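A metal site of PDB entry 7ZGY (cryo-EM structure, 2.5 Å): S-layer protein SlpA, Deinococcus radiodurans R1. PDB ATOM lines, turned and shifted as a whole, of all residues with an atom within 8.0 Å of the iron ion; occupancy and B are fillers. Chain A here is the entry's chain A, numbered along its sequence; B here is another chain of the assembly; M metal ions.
OD2 of Asp 438 sits at hydrogen-bond distance from N of Gly 443 (2.8 Å). The side-chain amide nitrogen of Asn 440 is in hydrogen-bond range of the side-chain carboxylate of Glu 449 (3.4 Å). OD1 of Asn 440 lies within hydrogen-bond range of OG1 of Thr 439 (3.0 Å). The side-chain carboxylate of Glu 449 lies within hydrogen-bond range of the side-chain hydroxyl of Thr 439 (2.8 Å). The side-chain amide nitrogen (ND2) of Asn 442 lies close to the side-chain carboxylate (OD1) of Asp 446 (2.7 Å). The side-chain carboxylate (OD2) of Asp 438 sits at hydrogen-bond distance from the backbone NH (N) of Gly 441 (3.4 Å).
Merely in contact with the iron ion: Glu 449 (3.3 Å) and Asn 440 (3.9 Å). Within 4 Å of the iron ion: Asp 438, Asn 440, Asn 442, Lys 444, Asp 446 and Glu 449.
The iron ion is bound by the side-chain amide oxygen of Asn 442 (2.1 Å), the backbone carbonyl oxygen of Lys 444 (2.3 Å), the side-chain carboxylate of Asp 438 (2.5 Å) and the side-chain amide nitrogen of Asn 442 (2.5 Å). Slightly farther from the iron ion lies OD2 of Asp 446 (2.8 Å).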
ATOM      1  N   TYR A 436      11.876  33.398  21.281  1.00  0.00           N
ATOM      2  CA  TYR A 436      11.681  31.974  21.468  1.00  0.00           C
ATOM      3  C   TYR A 436      12.068  31.607  22.893  1.00  0.00           C
ATOM      4  O   TYR A 436      12.737  32.361  23.592  1.00  0.00           O
ATOM      5  CB  TYR A 436      12.512  31.149  20.467  1.00  0.00           C
ATOM      6  CG  TYR A 436      13.991  31.439  20.544  1.00  0.00           C
ATOM      7  CD1 TYR A 436      14.537  32.524  19.896  1.00  0.00           C
ATOM      8  CD2 TYR A 436      14.840  30.607  21.275  1.00  0.00           C
ATOM      9  CE1 TYR A 436      15.891  32.789  19.975  1.00  0.00           C
ATOM     10  CE2 TYR A 436      16.186  30.872  21.361  1.00  0.00           C
ATOM     11  CZ  TYR A 436      16.704  31.960  20.694  1.00  0.00           C
ATOM     12  OH  TYR A 436      18.050  32.225  20.779  1.00  0.00           O
ATOM     13  N   VAL A 437      11.618  30.427  23.323  1.00  0.00           N
ATOM     14  CA  VAL A 437      11.935  29.906  24.641  1.00  0.00           C
ATOM     15  C   VAL A 437      13.087  28.913  24.493  1.00  0.00           C
ATOM     16  O   VAL A 437      12.919  27.849  23.901  1.00  0.00           O
ATOM     17  CB  VAL A 437      10.710  29.245  25.297  1.00  0.00           C
ATOM     18  CG1 VAL A 437      11.087  28.662  26.660  1.00  0.00           C
ATOM     19  CG2 VAL A 437       9.575  30.247  25.436  1.00  0.00           C
ATOM     20  N   ASP A 438      14.243  29.274  25.035  1.00  0.00           N
ATOM     21  CA  ASP A 438      15.442  28.455  24.913  1.00  0.00           C
ATOM     22  C   ASP A 438      15.468  27.438  26.053  1.00  0.00           C
ATOM     23  O   ASP A 438      15.863  27.757  27.179  1.00  0.00           O
ATOM     24  CB  ASP A 438      16.682  29.335  24.944  1.00  0.00           C
ATOM     25  CG  ASP A 438      17.896  28.641  24.354  1.00  0.00           C
ATOM     26  OD1 ASP A 438      17.740  27.920  23.355  1.00  0.00           O
ATOM     27  OD2 ASP A 438      19.009  28.842  24.889  1.00  0.00           O
ATOM     28  N   THR A 439      15.039  26.214  25.760  1.00  0.00           N
ATOM     29  CA  THR A 439      14.963  25.156  26.768  1.00  0.00           C
ATOM     30  C   THR A 439      16.246  24.348  26.886  1.00  0.00           C
ATOM     31  O   THR A 439      16.344  23.516  27.792  1.00  0.00           O
ATOM     32  CB  THR A 439      13.783  24.221  26.456  1.00  0.00           C
ATOM     33  OG1 THR A 439      13.961  23.654  25.153  1.00  0.00           O
ATOM     34  CG2 THR A 439      12.477  24.971  26.504  1.00  0.00           C
ATOM     35  N   ASN A 440      17.214  24.564  25.997  1.00  0.00           N
ATOM     36  CA  ASN A 440      18.461  23.807  26.019  1.00  0.00           C
ATOM     37  C   ASN A 440      19.643  24.587  26.578  1.00  0.00           C
ATOM     38  O   ASN A 440      20.570  23.975  27.101  1.00  0.00           O
ATOM     39  CB  ASN A 440      18.811  23.328  24.612  1.00  0.00           C
ATOM     40  CG  ASN A 440      17.668  22.596  23.939  1.00  0.00           C
ATOM     41  OD1 ASN A 440      16.642  22.328  24.559  1.00  0.00           O
ATOM     42  ND2 ASN A 440      17.846  22.256  22.669  1.00  0.00           N
ATOM     43  N   GLY A 441      19.627  25.917  26.478  1.00  0.00           N
ATOM     44  CA  GLY A 441      20.735  26.734  26.909  1.00  0.00           C
ATOM     45  C   GLY A 441      21.736  27.067  25.835  1.00  0.00           C
ATOM     46  O   GLY A 441      22.671  27.820  26.094  1.00  0.00           O
ATOM     47  N   ASN A 442      21.570  26.512  24.628  1.00  0.00           N
ATOM     48  CA  ASN A 442      22.520  26.793  23.553  1.00  0.00           C
ATOM     49  C   ASN A 442      22.502  28.255  23.141  1.00  0.00           C
ATOM     50  O   ASN A 442      23.433  28.731  22.482  1.00  0.00           O
ATOM     51  CB  ASN A 442      22.229  25.891  22.347  1.00  0.00           C
ATOM     52  CG  ASN A 442      20.767  25.931  21.934  1.00  0.00           C
ATOM     53  OD1 ASN A 442      19.971  26.668  22.508  1.00  0.00           O
ATOM     54  ND2 ASN A 442      20.420  25.129  20.933  1.00  0.00           N
ATOM     55  N   GLY A 443      21.442  28.984  23.505  1.00  0.00           N
ATOM     56  CA  GLY A 443      21.296  30.359  23.092  1.00  0.00           C
ATOM     57  C   GLY A 443      20.801  30.547  21.674  1.00  0.00           C
ATOM     58  O   GLY A 443      20.808  31.673  21.179  1.00  0.00           O
ATOM     59  N   LYS A 444      20.386  29.470  21.009  1.00  0.00           N
ATOM     60  CA  LYS A 444      19.914  29.518  19.637  1.00  0.00           C
ATOM     61  C   LYS A 444      18.591  28.768  19.532  1.00  0.00           C
ATOM     62  O   LYS A 444      18.312  27.871  20.329  1.00  0.00           O
ATOM     63  CB  LYS A 444      20.928  28.916  18.676  1.00  0.00           C
ATOM     64  CG  LYS A 444      21.111  27.415  18.845  1.00  0.00           C
ATOM     65  CD  LYS A 444      22.145  26.859  17.893  1.00  0.00           C
ATOM     66  CE  LYS A 444      22.342  25.371  18.111  1.00  0.00           C
ATOM     67  NZ  LYS A 444      21.124  24.601  17.750  1.00  0.00           N
ATOM     68  N   LYS A 445      17.788  29.151  18.549  1.00  0.00           N
ATOM     69  CA  LYS A 445      16.469  28.549  18.352  1.00  0.00           C
ATOM     70  C   LYS A 445      16.630  27.219  17.628  1.00  0.00           C
ATOM     71  O   LYS A 445      16.952  27.187  16.431  1.00  0.00           O
ATOM     72  CB  LYS A 445      15.560  29.496  17.576  1.00  0.00           C
ATOM     73  CG  LYS A 445      14.160  28.958  17.338  1.00  0.00           C
ATOM     74  CD  LYS A 445      13.281  29.994  16.667  1.00  0.00           C
ATOM     75  CE  LYS A 445      11.978  29.383  16.179  1.00  0.00           C
ATOM     76  NZ  LYS A 445      11.144  28.874  17.306  1.00  0.00           N
ATOM     77  N   ASP A 446      16.393  26.125  18.332  1.00  0.00           N
ATOM     78  CA  ASP A 446      16.466  24.792  17.757  1.00  0.00           C
ATOM     79  C   ASP A 446      15.194  24.544  16.952  1.00  0.00           C
ATOM     80  O   ASP A 446      14.438  25.469  16.634  1.00  0.00           O
ATOM     81  CB  ASP A 446      16.680  23.745  18.844  1.00  0.00           C
ATOM     82  CG  ASP A 446      18.055  23.830  19.471  1.00  0.00           C
ATOM     83  OD1 ASP A 446      18.995  24.273  18.775  1.00  0.00           O
ATOM     84  OD2 ASP A 446      18.198  23.462  20.648  1.00  0.00           O
ATOM     85  N   ASP A 447      14.931  23.288  16.596  1.00  0.00           N
ATOM     86  CA  ASP A 447      13.761  22.982  15.792  1.00  0.00           C
ATOM     87  C   ASP A 447      12.486  23.299  16.565  1.00  0.00           C
ATOM     88  O   ASP A 447      12.119  22.577  17.492  1.00  0.00           O
ATOM     89  CB  ASP A 447      13.767  21.507  15.375  1.00  0.00           C
ATOM     90  CG  ASP A 447      14.855  21.190  14.378  1.00  0.00           C
ATOM     91  OD1 ASP A 447      15.259  22.105  13.630  1.00  0.00           O
ATOM     92  OD2 ASP A 447      15.303  20.025  14.335  1.00  0.00           O
ATOM     93  N   GLU A 449      11.400  25.708  18.917  1.00  0.00           N
ATOM     94  CA  GLU A 449      11.589  25.668  20.348  1.00  0.00           C
ATOM     95  C   GLU A 449      10.317  26.068  21.092  1.00  0.00           C
ATOM     96  O   GLU A 449       9.690  25.220  21.734  1.00  0.00           O
ATOM     97  CB  GLU A 449      12.736  26.599  20.765  1.00  0.00           C
ATOM     98  CG  GLU A 449      14.126  26.012  20.613  1.00  0.00           C
ATOM     99  CD  GLU A 449      14.521  25.146  21.803  1.00  0.00           C
ATOM    100  OE1 GLU A 449      14.006  25.387  22.901  1.00  0.00           O
ATOM    101  OE2 GLU A 449      15.353  24.234  21.618  1.00  0.00           O
ATOM    102  N   ARG B 467      14.007  34.256  24.981  1.00  0.00           N
ATOM    103  CA  ARG B 467      15.199  34.893  24.462  1.00  0.00           C
ATOM    104  C   ARG B 467      14.918  35.470  23.076  1.00  0.00           C
ATOM    105  O   ARG B 467      13.869  35.241  22.476  1.00  0.00           O
ATOM    106  CB  ARG B 467      16.377  33.911  24.395  1.00  0.00           C
ATOM    107  CG  ARG B 467      17.726  34.547  24.094  1.00  0.00           C
ATOM    108  CD  ARG B 467      18.803  33.497  23.947  1.00  0.00           C
ATOM    109  NE  ARG B 467      19.102  32.837  25.209  1.00  0.00           N
ATOM    110  CZ  ARG B 467      19.924  33.308  26.136  1.00  0.00           C
ATOM    111  NH1 ARG B 467      20.544  34.468  25.973  1.00  0.00           N
ATOM    112  NH2 ARG B 467      20.137  32.612  27.239  1.00  0.00           N
HETATM  113 FE    FE M   1      18.169  26.043  21.705  1.00  0.00          FE
